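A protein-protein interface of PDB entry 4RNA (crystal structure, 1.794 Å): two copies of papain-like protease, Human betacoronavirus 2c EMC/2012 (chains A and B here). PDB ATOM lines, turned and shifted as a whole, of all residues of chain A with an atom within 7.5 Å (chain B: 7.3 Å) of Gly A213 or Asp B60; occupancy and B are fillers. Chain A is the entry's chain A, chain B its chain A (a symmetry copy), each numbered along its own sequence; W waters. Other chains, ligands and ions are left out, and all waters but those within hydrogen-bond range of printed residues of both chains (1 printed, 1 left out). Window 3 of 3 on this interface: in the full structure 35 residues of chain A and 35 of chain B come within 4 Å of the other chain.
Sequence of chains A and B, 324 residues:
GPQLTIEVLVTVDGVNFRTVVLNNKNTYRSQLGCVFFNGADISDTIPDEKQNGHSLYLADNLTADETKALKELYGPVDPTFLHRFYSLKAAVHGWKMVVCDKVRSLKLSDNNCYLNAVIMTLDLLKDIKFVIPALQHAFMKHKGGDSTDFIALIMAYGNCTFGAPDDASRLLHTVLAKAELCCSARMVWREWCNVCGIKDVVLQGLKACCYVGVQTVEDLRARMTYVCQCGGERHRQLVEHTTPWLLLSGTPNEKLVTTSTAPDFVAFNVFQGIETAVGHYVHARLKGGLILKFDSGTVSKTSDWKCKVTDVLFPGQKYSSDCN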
ATOM      1  N   TYR A 211      -1.794  19.693 -20.538  1.00  0.00           N
ATOM      2  CA  TYR A 211      -0.733  19.984 -21.461  1.00  0.00           C
ATOM      3  C   TYR A 211      -0.908  21.408 -21.863  1.00  0.00           C
ATOM      4  O   TYR A 211      -2.015  21.789 -22.103  1.00  0.00           O
ATOM      5  CB  TYR A 211      -0.840  19.055 -22.679  1.00  0.00           C
ATOM      6  CG  TYR A 211       0.315  19.248 -23.642  1.00  0.00           C
ATOM      7  CD1 TYR A 211       0.261  20.203 -24.661  1.00  0.00           C
ATOM      8  CD2 TYR A 211       1.524  18.512 -23.498  1.00  0.00           C
ATOM      9  CE1 TYR A 211       1.350  20.383 -25.539  1.00  0.00           C
ATOM     10  CE2 TYR A 211       2.594  18.712 -24.367  1.00  0.00           C
ATOM     11  CZ  TYR A 211       2.498  19.628 -25.389  1.00  0.00           C
ATOM     12  OH  TYR A 211       3.560  19.814 -26.249  1.00  0.00           O
ATOM     13  N   VAL A 212       0.175  22.167 -21.846  1.00  0.00           N
ATOM     14  CA  VAL A 212       0.179  23.532 -22.272  1.00  0.00           C
ATOM     15  C   VAL A 212       0.909  23.686 -23.584  1.00  0.00           C
ATOM     16  O   VAL A 212       2.045  23.311 -23.693  1.00  0.00           O
ATOM     17  CB  VAL A 212       0.747  24.452 -21.181  1.00  0.00           C
ATOM     18  CG1 VAL A 212       0.852  25.879 -21.708  1.00  0.00           C
ATOM     19  CG2 VAL A 212      -0.195  24.362 -19.942  1.00  0.00           C
ATOM     20  N   GLY A 213       0.256  24.361 -24.542  1.00  0.00           N
ATOM     21  CA  GLY A 213       0.849  24.628 -25.832  1.00  0.00           C
ATOM     22  C   GLY A 213       0.044  24.134 -27.022  1.00  0.00           C
ATOM     23  O   GLY A 213       0.378  24.519 -28.156  1.00  0.00           O
ATOM     24  N   VAL A 214      -0.979  23.274 -26.803  1.00  0.00           N
ATOM     25  CA  VAL A 214      -1.959  22.938 -27.894  1.00  0.00           C
ATOM     26  C   VAL A 214      -3.319  23.004 -27.235  1.00  0.00           C
ATOM     27  O   VAL A 214      -3.438  22.956 -25.975  1.00  0.00           O
ATOM     28  CB  VAL A 214      -1.770  21.565 -28.659  1.00  0.00           C
ATOM     29  CG1 VAL A 214      -0.460  21.495 -29.495  1.00  0.00           C
ATOM     30  CG2 VAL A 214      -1.904  20.379 -27.709  1.00  0.00           C
ATOM     31  N   GLN A 215      -4.351  23.153 -28.076  1.00  0.00           N
ATOM     32  CA  GLN A 215      -5.729  23.229 -27.594  1.00  0.00           C
ATOM     33  C   GLN A 215      -6.644  22.162 -28.244  1.00  0.00           C
ATOM     34  O   GLN A 215      -7.877  22.169 -27.967  1.00  0.00           O
ATOM     35  CB  GLN A 215      -6.223  24.679 -27.846  1.00  0.00           C
ATOM     36  CG  GLN A 215      -5.553  25.697 -26.881  1.00  0.00           C
ATOM     37  CD  GLN A 215      -5.597  27.107 -27.388  1.00  0.00           C
ATOM     38  OE1 GLN A 215      -5.376  27.347 -28.573  1.00  0.00           O
ATOM     39  NE2 GLN A 215      -5.886  28.063 -26.507  1.00  0.00           N
ATOM     40  N   THR A 216      -6.064  21.219 -29.037  1.00  0.00           N
ATOM     41  CA  THR A 216      -6.881  20.117 -29.646  1.00  0.00           C
ATOM     42  C   THR A 216      -6.099  18.862 -29.495  1.00  0.00           C
ATOM     43  O   THR A 216      -4.880  18.958 -29.475  1.00  0.00           O
ATOM     44  CB  THR A 216      -7.260  20.284 -31.181  1.00  0.00           C
ATOM     45  OG1 THR A 216      -6.143  20.161 -32.052  1.00  0.00           O
ATOM     46  CG2 THR A 216      -7.830  21.697 -31.505  1.00  0.00           C
ATOM     47  N   ASP A 219      -3.924  18.325 -32.660  1.00  0.00           N
ATOM     48  CA  ASP A 219      -2.603  19.003 -32.505  1.00  0.00           C
ATOM     49  C   ASP A 219      -1.720  18.299 -31.534  1.00  0.00           C
ATOM     50  O   ASP A 219      -0.517  18.162 -31.795  1.00  0.00           O
ATOM     51  CB  ASP A 219      -2.731  20.474 -32.194  1.00  0.00           C
ATOM     52  CG  ASP A 219      -3.383  21.241 -33.353  1.00  0.00           C
ATOM     53  OD1 ASP A 219      -3.081  20.865 -34.514  1.00  0.00           O
ATOM     54  OD2 ASP A 219      -4.192  22.204 -33.144  1.00  0.00           O
ATOM     55  N   LEU A 220      -2.302  17.777 -30.461  1.00  0.00           N
ATOM     56  CA  LEU A 220      -1.499  17.124 -29.438  1.00  0.00           C
ATOM     57  C   LEU A 220      -0.801  15.924 -29.989  1.00  0.00           C
ATOM     58  O   LEU A 220       0.335  15.599 -29.562  1.00  0.00           O
ATOM     59  CB  LEU A 220      -2.348  16.684 -28.240  1.00  0.00           C
ATOM     60  CG  LEU A 220      -1.623  16.080 -27.083  1.00  0.00           C
ATOM     61  CD1 LEU A 220      -0.766  17.086 -26.278  1.00  0.00           C
ATOM     62  CD2 LEU A 220      -2.611  15.291 -26.208  1.00  0.00           C
ATOM     63  N   LEU A 248      -6.265  20.986 -21.891  1.00  0.00           N
ATOM     64  CA  LEU A 248      -5.269  21.585 -22.790  1.00  0.00           C
ATOM     65  C   LEU A 248      -5.351  23.084 -22.718  1.00  0.00           C
ATOM     66  O   LEU A 248      -6.453  23.582 -22.493  1.00  0.00           O
ATOM     67  CB  LEU A 248      -5.464  21.090 -24.258  1.00  0.00           C
ATOM     68  CG  LEU A 248      -5.502  19.598 -24.570  1.00  0.00           C
ATOM     69  CD1 LEU A 248      -5.784  19.282 -26.040  1.00  0.00           C
ATOM     70  CD2 LEU A 248      -4.156  19.037 -24.157  1.00  0.00           C
ATOM     71  N   SER A 249      -4.213  23.778 -22.737  1.00  0.00           N
ATOM     72  CA  SER A 249      -4.235  25.235 -22.616  1.00  0.00           C
ATOM     73  C   SER A 249      -3.318  25.911 -23.576  1.00  0.00           C
ATOM     74  O   SER A 249      -2.264  25.486 -23.813  1.00  0.00           O
ATOM     75  CB  SER A 249      -3.906  25.753 -21.176  1.00  0.00           C
ATOM     76  OG  SER A 249      -4.612  24.999 -20.231  1.00  0.00           O
ATOM     77  N   GLY A 250      -3.682  27.100 -24.076  1.00  0.00           N
ATOM     78  CA  GLY A 250      -2.700  27.913 -24.730  1.00  0.00           C
ATOM     79  C   GLY A 250      -3.177  29.367 -24.566  1.00  0.00           C
ATOM     80  O   GLY A 250      -4.139  29.602 -23.875  1.00  0.00           O
ATOM     81  N   THR A 251      -2.459  30.284 -25.165  1.00  0.00           N
ATOM     82  CA  THR A 251      -2.721  31.715 -25.022  1.00  0.00           C
ATOM     83  C   THR A 251      -3.956  31.920 -25.827  1.00  0.00           C
ATOM     84  O   THR A 251      -4.332  31.075 -26.666  1.00  0.00           O
ATOM     85  CB  THR A 251      -1.540  32.560 -25.610  1.00  0.00           C
ATOM     86  OG1 THR A 251      -1.310  32.146 -26.949  1.00  0.00           O
ATOM     87  CG2 THR A 251      -0.255  32.320 -24.873  1.00  0.00           C
ATOM     88  N   VAL B  12      14.767  28.361 -25.026  1.00  0.00           N
ATOM     89  CA  VAL B  12      14.086  28.821 -23.799  1.00  0.00           C
ATOM     90  C   VAL B  12      15.036  29.470 -22.786  1.00  0.00           C
ATOM     91  O   VAL B  12      14.608  30.038 -21.746  1.00  0.00           O
ATOM     92  CB  VAL B  12      13.296  27.707 -23.088  1.00  0.00           C
ATOM     93  CG1 VAL B  12      12.323  27.013 -24.009  1.00  0.00           C
ATOM     94  CG2 VAL B  12      14.235  26.663 -22.392  1.00  0.00           C
ATOM     95  N   ARG B  18      17.860  25.069 -30.796  1.00  0.00           N
ATOM     96  CA  ARG B  18      17.579  24.068 -31.820  1.00  0.00           C
ATOM     97  C   ARG B  18      17.145  24.719 -33.051  1.00  0.00           C
ATOM     98  O   ARG B  18      16.423  25.797 -33.015  1.00  0.00           O
ATOM     99  CB  ARG B  18      16.563  22.983 -31.400  1.00  0.00           C
ATOM    100  CG  ARG B  18      15.215  23.501 -31.084  1.00  0.00           C
ATOM    101  CD  ARG B  18      14.169  22.397 -30.942  1.00  0.00           C
ATOM    102  NE  ARG B  18      12.990  22.965 -30.271  1.00  0.00           N
ATOM    103  CZ  ARG B  18      11.733  22.835 -30.656  1.00  0.00           C
ATOM    104  NH1 ARG B  18      11.438  22.141 -31.741  1.00  0.00           N
ATOM    105  NH2 ARG B  18      10.777  23.385 -29.919  1.00  0.00           N
ATOM    106  N   ARG B  29       2.425  29.801 -34.188  1.00  0.00           N
ATOM    107  CA  ARG B  29       1.638  28.973 -33.273  1.00  0.00           C
ATOM    108  C   ARG B  29       1.316  27.588 -33.836  1.00  0.00           C
ATOM    109  O   ARG B  29       1.614  26.551 -33.195  1.00  0.00           O
ATOM    110  CB  ARG B  29       0.358  29.687 -32.847  1.00  0.00           C
ATOM    111  CG  ARG B  29      -0.424  28.801 -31.849  1.00  0.00           C
ATOM    112  CD  ARG B  29      -1.901  29.162 -31.683  1.00  0.00           C
ATOM    113  NE  ARG B  29      -2.072  30.560 -31.378  1.00  0.00           N
ATOM    114  CZ  ARG B  29      -2.383  31.017 -30.168  1.00  0.00           C
ATOM    115  NH1 ARG B  29      -2.552  30.165 -29.141  1.00  0.00           N
ATOM    116  NH2 ARG B  29      -2.582  32.329 -30.000  1.00  0.00           N
ATOM    117  N   LEU B  32       4.785  25.679 -34.409  1.00  0.00           N
ATOM    118  CA  LEU B  32       5.817  25.577 -33.330  1.00  0.00           C
ATOM    119  C   LEU B  32       5.220  25.793 -31.936  1.00  0.00           C
ATOM    120  O   LEU B  32       5.299  24.947 -31.071  1.00  0.00           O
ATOM    121  CB  LEU B  32       6.908  26.597 -33.642  1.00  0.00           C
ATOM    122  CG  LEU B  32       8.193  26.748 -32.877  1.00  0.00           C
ATOM    123  CD1 LEU B  32       8.941  25.395 -32.825  1.00  0.00           C
ATOM    124  CD2 LEU B  32       9.009  27.913 -33.532  1.00  0.00           C
ATOM    125  N   GLY B  33       4.597  26.935 -31.702  1.00  0.00           N
ATOM    126  CA  GLY B  33       4.006  27.155 -30.373  1.00  0.00           C
ATOM    127  C   GLY B  33       4.027  28.639 -30.124  1.00  0.00           C
ATOM    128  O   GLY B  33       4.187  29.390 -31.103  1.00  0.00           O
ATOM    129  N   CYS B  34       3.894  29.039 -28.857  1.00  0.00           N
ATOM    130  CA  CYS B  34       3.892  30.440 -28.445  1.00  0.00           C
ATOM    131  C   CYS B  34       5.345  30.923 -28.482  1.00  0.00           C
ATOM    132  O   CYS B  34       6.209  30.359 -27.798  1.00  0.00           O
ATOM    133  CB  CYS B  34       3.362  30.585 -27.020  1.00  0.00           C
ATOM    134  SG  CYS B  34       3.419  32.334 -26.513  1.00  0.00           S
ATOM    135  N   VAL B  35       5.600  31.960 -29.268  1.00  0.00           N
ATOM    136  CA  VAL B  35       7.005  32.387 -29.478  1.00  0.00           C
ATOM    137  C   VAL B  35       7.130  33.890 -29.353  1.00  0.00           C
ATOM    138  O   VAL B  35       6.268  34.668 -29.829  1.00  0.00           O
ATOM    139  CB  VAL B  35       7.567  31.963 -30.881  1.00  0.00           C
ATOM    140  CG1 VAL B  35       7.915  30.485 -30.945  1.00  0.00           C
ATOM    141  CG2 VAL B  35       6.577  32.334 -31.961  1.00  0.00           C
ATOM    142  N   SER B  43       3.249  34.757 -32.094  1.00  0.00           N
ATOM    143  CA  SER B  43       2.667  33.413 -32.337  1.00  0.00           C
ATOM    144  C   SER B  43       1.671  33.392 -33.498  1.00  0.00           C
ATOM    145  O   SER B  43       1.617  32.450 -34.240  1.00  0.00           O
ATOM    146  CB  SER B  43       1.925  32.836 -31.108  1.00  0.00           C
ATOM    147  OG  SER B  43       2.762  32.867 -29.944  1.00  0.00           O
ATOM    148  N   TYR B  57      12.311  32.946 -28.973  1.00  0.00           N
ATOM    149  CA  TYR B  57      12.104  32.507 -27.586  1.00  0.00           C
ATOM    150  C   TYR B  57      10.834  31.702 -27.467  1.00  0.00           C
ATOM    151  O   TYR B  57       9.793  32.203 -27.628  1.00  0.00           O
ATOM    152  CB  TYR B  57      12.105  33.715 -26.638  1.00  0.00           C
ATOM    153  CG  TYR B  57      13.482  33.937 -26.205  1.00  0.00           C
ATOM    154  CD1 TYR B  57      14.346  34.718 -26.967  1.00  0.00           C
ATOM    155  CD2 TYR B  57      13.970  33.279 -25.064  1.00  0.00           C
ATOM    156  CE1 TYR B  57      15.679  34.864 -26.581  1.00  0.00           C
ATOM    157  CE2 TYR B  57      15.280  33.455 -24.650  1.00  0.00           C
ATOM    158  CZ  TYR B  57      16.124  34.212 -25.430  1.00  0.00           C
ATOM    159  OH  TYR B  57      17.415  34.348 -24.981  1.00  0.00           O
ATOM    160  N   LEU B  58      10.915  30.406 -27.240  1.00  0.00           N
ATOM    161  CA  LEU B  58       9.685  29.571 -27.201  1.00  0.00           C
ATOM    162  C   LEU B  58       9.071  29.584 -25.774  1.00  0.00           C
ATOM    163  O   LEU B  58       9.809  29.517 -24.774  1.00  0.00           O
ATOM    164  CB  LEU B  58      10.011  28.114 -27.595  1.00  0.00           C
ATOM    165  CG  LEU B  58       8.815  27.127 -27.676  1.00  0.00           C
ATOM    166  CD1 LEU B  58       7.729  27.484 -28.753  1.00  0.00           C
ATOM    167  CD2 LEU B  58       9.402  25.766 -27.995  1.00  0.00           C
ATOM    168  N   ALA B  59       7.742  29.705 -25.650  1.00  0.00           N
ATOM    169  CA  ALA B  59       7.091  29.800 -24.297  1.00  0.00           C
ATOM    170  C   ALA B  59       6.304  28.502 -23.969  1.00  0.00           C
ATOM    171  O   ALA B  59       5.937  28.299 -22.827  1.00  0.00           O
ATOM    172  CB  ALA B  59       6.192  31.040 -24.157  1.00  0.00           C
ATOM    173  N   ASP B  60       6.032  27.620 -24.950  1.00  0.00           N
ATOM    174  CA  ASP B  60       5.226  26.388 -24.659  1.00  0.00           C
ATOM    175  C   ASP B  60       5.444  25.436 -25.763  1.00  0.00           C
ATOM    176  O   ASP B  60       6.154  25.758 -26.697  1.00  0.00           O
ATOM    177  CB  ASP B  60       3.703  26.640 -24.362  1.00  0.00           C
ATOM    178  CG  ASP B  60       2.937  27.308 -25.561  1.00  0.00           C
ATOM    179  OD1 ASP B  60       3.362  27.135 -26.747  1.00  0.00           O
ATOM    180  OD2 ASP B  60       1.891  27.994 -25.303  1.00  0.00           O
ATOM    181  N   ASN B  61       4.977  24.197 -25.599  1.00  0.00           N
ATOM    182  CA  ASN B  61       5.365  23.136 -26.513  1.00  0.00           C
ATOM    183  C   ASN B  61       6.799  22.699 -26.562  1.00  0.00           C
ATOM    184  O   ASN B  61       7.263  22.428 -27.659  1.00  0.00           O
ATOM    185  CB  ASN B  61       5.051  23.520 -27.943  1.00  0.00           C
ATOM    186  CG  ASN B  61       3.689  23.236 -28.241  1.00  0.00           C
ATOM    187  OD1 ASN B  61       2.937  24.162 -28.552  1.00  0.00           O
ATOM    188  ND2 ASN B  61       3.284  21.984 -28.010  1.00  0.00           N
ATOM    189  N   LEU B  62       7.448  22.499 -25.403  1.00  0.00           N
ATOM    190  CA  LEU B  62       8.862  22.478 -25.376  1.00  0.00           C
ATOM    191  C   LEU B  62       9.146  20.981 -25.515  1.00  0.00           C
ATOM    192  O   LEU B  62       8.316  20.153 -25.082  1.00  0.00           O
ATOM    193  CB  LEU B  62       9.390  22.944 -23.981  1.00  0.00           C
ATOM    194  CG  LEU B  62       9.071  24.278 -23.277  1.00  0.00           C
ATOM    195  CD1 LEU B  62      10.062  24.542 -22.132  1.00  0.00           C
ATOM    196  CD2 LEU B  62       8.842  25.522 -24.155  1.00  0.00           C
ATOM    197  N   THR B  63      10.281  20.697 -26.112  1.00  0.00           N
ATOM    198  CA  THR B  63      10.852  19.346 -26.219  1.00  0.00           C
ATOM    199  C   THR B  63      11.334  18.899 -24.861  1.00  0.00           C
ATOM    200  O   THR B  63      11.398  19.691 -23.897  1.00  0.00           O
ATOM    201  CB  THR B  63      12.048  19.378 -27.175  1.00  0.00           C
ATOM    202  OG1 THR B  63      13.029  20.292 -26.642  1.00  0.00           O
ATOM    203  CG2 THR B  63      11.641  19.918 -28.579  1.00  0.00           C
ATOM    204  N   GLU B  66      14.327  20.956 -23.948  1.00  0.00           N
ATOM    205  CA  GLU B  66      14.011  22.300 -23.494  1.00  0.00           C
ATOM    206  C   GLU B  66      13.415  22.309 -22.078  1.00  0.00           C
ATOM    207  O   GLU B  66      13.698  23.227 -21.304  1.00  0.00           O
ATOM    208  CB  GLU B  66      13.071  22.982 -24.478  1.00  0.00           C
ATOM    209  CG  GLU B  66      13.807  23.356 -25.751  1.00  0.00           C
ATOM    210  CD  GLU B  66      12.857  23.627 -26.918  1.00  0.00           C
ATOM    211  OE1 GLU B  66      11.723  23.098 -26.886  1.00  0.00           O
ATOM    212  OE2 GLU B  66      13.304  24.316 -27.900  1.00  0.00           O
ATOM    213  N   PRO B  79       3.492  25.975 -15.978  1.00  0.00           N
ATOM    214  CA  PRO B  79       3.605  25.926 -17.413  1.00  0.00           C
ATOM    215  C   PRO B  79       3.339  27.288 -17.980  1.00  0.00           C
ATOM    216  O   PRO B  79       3.724  27.547 -19.119  1.00  0.00           O
ATOM    217  CB  PRO B  79       2.510  24.929 -17.835  1.00  0.00           C
ATOM    218  CG  PRO B  79       1.630  24.722 -16.661  1.00  0.00           C
ATOM    219  CD  PRO B  79       2.402  25.122 -15.443  1.00  0.00           C
ATOM    220  N   LEU B  82       6.968  30.947 -18.503  1.00  0.00           N
ATOM    221  CA  LEU B  82       7.711  31.667 -19.571  1.00  0.00           C
ATOM    222  C   LEU B  82       6.867  32.749 -20.165  1.00  0.00           C
ATOM    223  O   LEU B  82       7.413  33.864 -20.400  1.00  0.00           O
ATOM    224  CB  LEU B  82       8.167  30.813 -20.720  1.00  0.00           C
ATOM    225  CG  LEU B  82       9.326  29.898 -20.307  1.00  0.00           C
ATOM    226  CD1 LEU B  82       9.731  28.732 -21.282  1.00  0.00           C
ATOM    227  CD2 LEU B  82      10.544  30.740 -19.858  1.00  0.00           C
ATOM    228  N   HIS B  83       5.623  32.398 -20.489  1.00  0.00           N
ATOM    229  CA  HIS B  83       4.777  33.487 -21.101  1.00  0.00           C
ATOM    230  C   HIS B  83       4.740  34.662 -20.183  1.00  0.00           C
ATOM    231  O   HIS B  83       4.690  35.876 -20.631  1.00  0.00           O
ATOM    232  CB  HIS B  83       3.350  33.040 -21.436  1.00  0.00           C
ATOM    233  CG  HIS B  83       2.567  34.134 -22.205  1.00  0.00           C
ATOM    234  ND1 HIS B  83       1.769  35.040 -21.580  1.00  0.00           N
ATOM    235  CD2 HIS B  83       2.554  34.474 -23.568  1.00  0.00           C
ATOM    236  CE1 HIS B  83       1.258  35.915 -22.500  1.00  0.00           C
ATOM    237  NE2 HIS B  83       1.740  35.567 -23.713  1.00  0.00           N
ATOM    238  N   TYR B  86       8.132  36.593 -20.043  1.00  0.00           N
ATOM    239  CA  TYR B  86       8.550  37.276 -21.212  1.00  0.00           C
ATOM    240  C   TYR B  86       7.670  38.486 -21.315  1.00  0.00           C
ATOM    241  O   TYR B  86       8.224  39.513 -21.630  1.00  0.00           O
ATOM    242  CB  TYR B  86       8.373  36.493 -22.535  1.00  0.00           C
ATOM    243  CG  TYR B  86       9.247  35.215 -22.685  1.00  0.00           C
ATOM    244  CD1 TYR B  86      10.471  35.093 -22.015  1.00  0.00           C
ATOM    245  CD2 TYR B  86       8.856  34.202 -23.548  1.00  0.00           C
ATOM    246  CE1 TYR B  86      11.247  33.933 -22.158  1.00  0.00           C
ATOM    247  CE2 TYR B  86       9.641  33.034 -23.699  1.00  0.00           C
ATOM    248  CZ  TYR B  86      10.824  32.935 -23.000  1.00  0.00           C
ATOM    249  OH  TYR B  86      11.543  31.733 -23.170  1.00  0.00           O
HETATM  250  O   HOH W   1      -0.208  28.967 -26.522  1.00  0.00           O
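The side-chain amide nitrogen (ND2) of Asn B61 lies within hydrogen-bond range of the side-chain hydroxyl (OH) of Tyr A211, at 2.8 Å.
The side-chain amide oxygen of Asn B61 lies close to the backbone carbonyl oxygen of Gly A213.
O of Thr A251 is in hydrogen-bond range of NH1 of Arg B29, 3.2 Å away.
The backbone carbonyl oxygen (O) of Tyr A211 sits at hydrogen-bond distance from the backbone NH (N) of Ser A249 (3.0 Å).
N of Gly A213 sits at hydrogen-bond distance from O of Ser A249, 2.9 Å away.
NE2 of Gln A215 lies within hydrogen-bond range of O of Thr A251, 3.4 Å away.
The backbone NH (N) of Arg B29 sits at hydrogen-bond distance from the backbone carbonyl oxygen (O) of Ser B43 (2.8 Å).
The backbone NH of Cys B34 is in hydrogen-bond range of the side-chain carboxylate of Asp B60, 2.9 Å away.
Among the printed residues, pairs that only touch across the chains: Gly A213 with Asp B60, Val A212 with Pro B79, Val A212 with Asn B61, Thr A251 with His B83 and Val A212 with Asp B60.
Of chain A, only Val A212 and Gly A213 come within 4 Å of Asp B60.
Of the printed residues of chain B, Thr A251 touches Arg B29 and His B83.
Of the printed residues of chain B, Tyr A211 touches Asn B61.
Of the 12 printed residues of chain A, 4 touch a printed residue of chain B.
Printed residues of chain A that touch a printed residue of chain B: Tyr A211, Val A212, Gly A213 and Thr A251.
Hydrophobic or aromatic side chains of chain A that line the printed part of chain B: Tyr A211 and Val A212.
Printed residues of chain B that touch a printed residue of chain A: Arg B29, Asp B60, Asn B61, Pro B79 and His B83.
Hydrophobic or aromatic side chains of chain B within 4 Å of the printed part of chain A: Pro B79 and His B83.
Among the printed residues, 8 pairs touch across the chains.
No position is printed for both chains.
Of the 8 pairs that touch across the chains among the printed residues, none has its exchanged pair printed and touching as well.
Water W1 lies within hydrogen-bond range of the side-chain carboxylate of Asp B60 (2.6 Å) and the backbone NH of Thr A251 (2.9 Å).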
